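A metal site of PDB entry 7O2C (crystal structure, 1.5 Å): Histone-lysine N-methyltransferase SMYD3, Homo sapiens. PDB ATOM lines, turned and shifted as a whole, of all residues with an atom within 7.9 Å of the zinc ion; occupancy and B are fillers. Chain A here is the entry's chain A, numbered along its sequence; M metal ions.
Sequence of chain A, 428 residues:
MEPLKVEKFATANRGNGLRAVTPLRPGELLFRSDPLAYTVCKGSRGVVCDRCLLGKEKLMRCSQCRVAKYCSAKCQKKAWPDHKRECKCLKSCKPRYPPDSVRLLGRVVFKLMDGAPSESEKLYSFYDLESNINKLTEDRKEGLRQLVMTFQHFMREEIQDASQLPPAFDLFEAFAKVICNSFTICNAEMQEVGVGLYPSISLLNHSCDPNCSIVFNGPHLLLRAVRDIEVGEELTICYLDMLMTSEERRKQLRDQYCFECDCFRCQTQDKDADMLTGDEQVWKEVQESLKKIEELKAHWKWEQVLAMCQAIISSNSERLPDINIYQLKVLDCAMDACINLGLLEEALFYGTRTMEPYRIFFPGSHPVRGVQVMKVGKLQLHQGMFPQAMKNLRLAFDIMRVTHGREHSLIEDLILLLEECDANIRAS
The side-chain hydroxyl of Ser 72 sits close to the side-chain sulfur of Cys 71.
The side-chain hydroxyl (OG) of Ser 72 lies within hydrogen-bond range of the backbone NH (N) of Cys 75 (3.0 Å).
The backbone NH (N) of Leu 54 lies close to the side-chain sulfur (SG) of Cys 52 (3.8 Å).
The side-chain sulfur (SG) of Cys 49 lies close to the backbone NH (N) of Arg 51 (3.5 Å).
The backbone NH (N) of Cys 49 sits at hydrogen-bond distance from the backbone carbonyl oxygen (O) of Leu 54 (2.9 Å).
The zinc ion is bound by the side-chain sulfur (SG) of Cys 71, the side-chain sulfur (SG) of Cys 75, the side-chain sulfur (SG) of Cys 52 and the side-chain sulfur (SG) of Cys 49.
Of the 18 residues printed, 4 come within 4 Å of the zinc ion.
The nearest printed residue that does not touch the zinc ion is Ser 72 (4.3 Å).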
ATOM      1  N   VAL A  48      25.711   1.187 -19.371  1.00  0.00           N
ATOM      2  CA  VAL A  48      26.679   0.657 -20.375  1.00  0.00           C
ATOM      3  C   VAL A  48      25.903   0.029 -21.523  1.00  0.00           C
ATOM      4  O   VAL A  48      24.739  -0.327 -21.349  1.00  0.00           O
ATOM      5  CB  VAL A  48      27.674  -0.370 -19.792  1.00  0.00           C
ATOM      6  CG1 VAL A  48      28.415   0.147 -18.539  1.00  0.00           C
ATOM      7  CG2 VAL A  48      27.025  -1.713 -19.540  1.00  0.00           C
ATOM      8  N   CYS A  49      26.559  -0.007 -22.687  1.00  0.00           N
ATOM      9  CA  CYS A  49      26.019  -0.561 -23.923  1.00  0.00           C
ATOM     10  C   CYS A  49      25.721  -2.060 -23.705  1.00  0.00           C
ATOM     11  O   CYS A  49      26.610  -2.787 -23.262  1.00  0.00           O
ATOM     12  CB  CYS A  49      26.994  -0.333 -25.075  1.00  0.00           C
ATOM     13  SG  CYS A  49      26.461  -1.087 -26.628  1.00  0.00           S
ATOM     14  N   ASP A  50      24.501  -2.501 -24.006  1.00  0.00           N
ATOM     15  CA  ASP A  50      24.149  -3.932 -23.864  1.00  0.00           C
ATOM     16  C   ASP A  50      25.128  -4.815 -24.624  1.00  0.00           C
ATOM     17  O   ASP A  50      25.350  -5.917 -24.159  1.00  0.00           O
ATOM     18  CB  ASP A  50      22.766  -4.210 -24.433  1.00  0.00           C
ATOM     19  CG  ASP A  50      21.653  -4.264 -23.415  1.00  0.00           C
ATOM     20  OD1 ASP A  50      21.535  -3.341 -22.577  1.00  0.00           O
ATOM     21  OD2 ASP A  50      20.920  -5.266 -23.455  1.00  0.00           O
ATOM     22  N   ARG A  51      25.602  -4.399 -25.796  1.00  0.00           N
ATOM     23  CA  ARG A  51      26.497  -5.219 -26.654  1.00  0.00           C
ATOM     24  C   ARG A  51      27.937  -5.083 -26.162  1.00  0.00           C
ATOM     25  O   ARG A  51      28.488  -6.086 -25.735  1.00  0.00           O
ATOM     26  CB  ARG A  51      26.399  -4.802 -28.119  1.00  0.00           C
ATOM     27  CG  ARG A  51      27.368  -5.558 -29.022  1.00  0.00           C
ATOM     28  CD  ARG A  51      26.687  -6.418 -30.050  1.00  0.00           C
ATOM     29  NE  ARG A  51      27.630  -7.191 -30.852  1.00  0.00           N
ATOM     30  CZ  ARG A  51      27.567  -8.486 -31.072  1.00  0.00           C
ATOM     31  NH1 ARG A  51      26.580  -9.209 -30.568  1.00  0.00           N
ATOM     32  NH2 ARG A  51      28.476  -9.050 -31.828  1.00  0.00           N
ATOM     33  N   CYS A  52      28.554  -3.904 -26.306  1.00  0.00           N
ATOM     34  CA  CYS A  52      30.033  -3.845 -26.079  1.00  0.00           C
ATOM     35  C   CYS A  52      30.387  -3.610 -24.602  1.00  0.00           C
ATOM     36  O   CYS A  52      31.629  -3.665 -24.303  1.00  0.00           O
ATOM     37  CB  CYS A  52      30.696  -2.831 -26.996  1.00  0.00           C
ATOM     38  SG  CYS A  52      30.238  -1.120 -26.613  1.00  0.00           S
ATOM     39  N   LEU A  53      29.407  -3.327 -23.714  1.00  0.00           N
ATOM     40  CA  LEU A  53      29.632  -3.146 -22.242  1.00  0.00           C
ATOM     41  C   LEU A  53      30.499  -1.935 -21.960  1.00  0.00           C
ATOM     42  O   LEU A  53      31.062  -1.880 -20.831  1.00  0.00           O
ATOM     43  CB  LEU A  53      30.217  -4.422 -21.587  1.00  0.00           C
ATOM     44  CG  LEU A  53      29.321  -5.645 -21.840  1.00  0.00           C
ATOM     45  CD1 LEU A  53      29.897  -6.891 -21.202  1.00  0.00           C
ATOM     46  CD2 LEU A  53      27.915  -5.430 -21.319  1.00  0.00           C
ATOM     47  N   LEU A  54      30.485  -0.951 -22.871  1.00  0.00           N
ATOM     48  CA  LEU A  54      31.288   0.298 -22.679  1.00  0.00           C
ATOM     49  C   LEU A  54      30.321   1.391 -22.252  1.00  0.00           C
ATOM     50  O   LEU A  54      29.159   1.342 -22.682  1.00  0.00           O
ATOM     51  CB  LEU A  54      32.013   0.722 -23.962  1.00  0.00           C
ATOM     52  CG  LEU A  54      33.071  -0.221 -24.536  1.00  0.00           C
ATOM     53  CD1 LEU A  54      33.731   0.441 -25.741  1.00  0.00           C
ATOM     54  CD2 LEU A  54      34.114  -0.642 -23.489  1.00  0.00           C
ATOM     55  N   GLY A  55      30.774   2.354 -21.456  1.00  0.00           N
ATOM     56  CA  GLY A  55      29.856   3.374 -20.930  1.00  0.00           C
ATOM     57  C   GLY A  55      29.763   4.584 -21.834  1.00  0.00           C
ATOM     58  O   GLY A  55      30.541   4.694 -22.816  1.00  0.00           O
ATOM     59  N   LYS A  56      28.789   5.445 -21.576  1.00  0.00           N
ATOM     60  CA  LYS A  56      28.597   6.667 -22.386  1.00  0.00           C
ATOM     61  C   LYS A  56      27.447   7.501 -21.825  1.00  0.00           C
ATOM     62  O   LYS A  56      26.456   6.902 -21.355  1.00  0.00           O
ATOM     63  CB  LYS A  56      28.281   6.343 -23.843  1.00  0.00           C
ATOM     64  CG  LYS A  56      28.356   7.576 -24.747  1.00  0.00           C
ATOM     65  CD  LYS A  56      28.596   7.249 -26.186  1.00  0.00           C
ATOM     66  CE  LYS A  56      29.751   6.287 -26.361  1.00  0.00           C
ATOM     67  NZ  LYS A  56      30.374   6.441 -27.694  1.00  0.00           N
ATOM     68  N   LEU A  59      23.125   6.836 -24.253  1.00  0.00           N
ATOM     69  CA  LEU A  59      22.754   5.531 -24.875  1.00  0.00           C
ATOM     70  C   LEU A  59      21.377   5.638 -25.543  1.00  0.00           C
ATOM     71  O   LEU A  59      20.456   6.331 -25.025  1.00  0.00           O
ATOM     72  CB  LEU A  59      22.709   4.407 -23.832  1.00  0.00           C
ATOM     73  CG  LEU A  59      24.009   4.076 -23.106  1.00  0.00           C
ATOM     74  CD1 LEU A  59      23.747   2.971 -22.113  1.00  0.00           C
ATOM     75  CD2 LEU A  59      25.142   3.704 -24.078  1.00  0.00           C
ATOM     76  N   LYS A  69      19.854  -1.064 -24.290  1.00  0.00           N
ATOM     77  CA  LYS A  69      20.403   0.271 -24.684  1.00  0.00           C
ATOM     78  C   LYS A  69      21.796   0.084 -25.258  1.00  0.00           C
ATOM     79  O   LYS A  69      22.506  -0.871 -24.894  1.00  0.00           O
ATOM     80  CB  LYS A  69      20.367   1.287 -23.539  1.00  0.00           C
ATOM     81  CG  LYS A  69      18.991   1.402 -22.937  1.00  0.00           C
ATOM     82  CD  LYS A  69      18.737   2.543 -21.995  1.00  0.00           C
ATOM     83  CE  LYS A  69      17.323   2.414 -21.452  1.00  0.00           C
ATOM     84  NZ  LYS A  69      17.174   2.881 -20.050  1.00  0.00           N
ATOM     85  N   TYR A  70      22.145   0.928 -26.205  1.00  0.00           N
ATOM     86  CA  TYR A  70      23.340   0.680 -27.031  1.00  0.00           C
ATOM     87  C   TYR A  70      24.090   1.998 -27.172  1.00  0.00           C
ATOM     88  O   TYR A  70      23.497   3.103 -27.088  1.00  0.00           O
ATOM     89  CB  TYR A  70      22.913   0.151 -28.384  1.00  0.00           C
ATOM     90  CG  TYR A  70      22.104  -1.101 -28.274  1.00  0.00           C
ATOM     91  CD1 TYR A  70      22.741  -2.317 -28.091  1.00  0.00           C
ATOM     92  CD2 TYR A  70      20.711  -1.085 -28.394  1.00  0.00           C
ATOM     93  CE1 TYR A  70      21.999  -3.497 -28.009  1.00  0.00           C
ATOM     94  CE2 TYR A  70      19.971  -2.238 -28.288  1.00  0.00           C
ATOM     95  CZ  TYR A  70      20.617  -3.437 -28.121  1.00  0.00           C
ATOM     96  OH  TYR A  70      19.926  -4.595 -28.051  1.00  0.00           O
ATOM     97  N   CYS A  71      25.386   1.837 -27.447  1.00  0.00           N
ATOM     98  CA  CYS A  71      26.308   2.980 -27.544  1.00  0.00           C
ATOM     99  C   CYS A  71      26.215   3.606 -28.937  1.00  0.00           C
ATOM    100  O   CYS A  71      26.619   4.765 -29.112  1.00  0.00           O
ATOM    101  CB  CYS A  71      27.720   2.547 -27.230  1.00  0.00           C
ATOM    102  SG  CYS A  71      28.523   1.562 -28.508  1.00  0.00           S
ATOM    103  N   SER A  72      25.758   2.871 -29.929  1.00  0.00           N
ATOM    104  CA  SER A  72      25.928   3.231 -31.352  1.00  0.00           C
ATOM    105  C   SER A  72      24.891   2.464 -32.182  1.00  0.00           C
ATOM    106  O   SER A  72      24.444   1.359 -31.756  1.00  0.00           O
ATOM    107  CB  SER A  72      27.319   2.848 -31.793  1.00  0.00           C
ATOM    108  OG  SER A  72      27.548   1.453 -31.593  1.00  0.00           O
ATOM    109  N   ALA A  73      24.627   2.945 -33.369  1.00  0.00           N
ATOM    110  CA  ALA A  73      23.800   2.169 -34.307  1.00  0.00           C
ATOM    111  C   ALA A  73      24.440   0.793 -34.555  1.00  0.00           C
ATOM    112  O   ALA A  73      23.636  -0.161 -34.727  1.00  0.00           O
ATOM    113  CB  ALA A  73      23.632   2.901 -35.614  1.00  0.00           C
ATOM    114  N   LYS A  74      25.758   0.737 -34.762  1.00  0.00           N
ATOM    115  CA  LYS A  74      26.504  -0.521 -35.031  1.00  0.00           C
ATOM    116  C   LYS A  74      26.140  -1.492 -33.905  1.00  0.00           C
ATOM    117  O   LYS A  74      25.793  -2.645 -34.200  1.00  0.00           O
ATOM    118  CB  LYS A  74      28.021  -0.267 -35.109  1.00  0.00           C
ATOM    119  CG  LYS A  74      28.937  -1.468 -35.309  1.00  0.00           C
ATOM    120  CD  LYS A  74      30.428  -1.102 -35.167  1.00  0.00           C
ATOM    121  CE  LYS A  74      31.443  -2.022 -35.815  1.00  0.00           C
ATOM    122  NZ  LYS A  74      30.975  -3.417 -35.968  1.00  0.00           N
ATOM    123  N   CYS A  75      26.262  -1.098 -32.641  1.00  0.00           N
ATOM    124  CA  CYS A  75      26.016  -2.047 -31.524  1.00  0.00           C
ATOM    125  C   CYS A  75      24.549  -2.463 -31.529  1.00  0.00           C
ATOM    126  O   CYS A  75      24.268  -3.684 -31.310  1.00  0.00           O
ATOM    127  CB  CYS A  75      26.435  -1.535 -30.155  1.00  0.00           C
ATOM    128  SG  CYS A  75      28.221  -1.672 -29.937  1.00  0.00           S
ATOM    129  N   GLN A  76      23.614  -1.544 -31.747  1.00  0.00           N
ATOM    130  CA  GLN A  76      22.164  -1.897 -31.657  1.00  0.00           C
ATOM    131  C   GLN A  76      21.844  -2.891 -32.771  1.00  0.00           C
ATOM    132  O   GLN A  76      21.123  -3.889 -32.527  1.00  0.00           O
ATOM    133  CB  GLN A  76      21.261  -0.668 -31.826  1.00  0.00           C
ATOM    134  CG  GLN A  76      19.782  -1.014 -31.750  1.00  0.00           C
ATOM    135  CD  GLN A  76      18.845   0.155 -31.532  1.00  0.00           C
ATOM    136  OE1 GLN A  76      19.265   1.273 -31.274  1.00  0.00           O
ATOM    137  NE2 GLN A  76      17.537  -0.104 -31.635  1.00  0.00           N
HETATM  138 ZN    ZN M   1      28.399  -0.613 -27.929  1.00  0.00          ZN
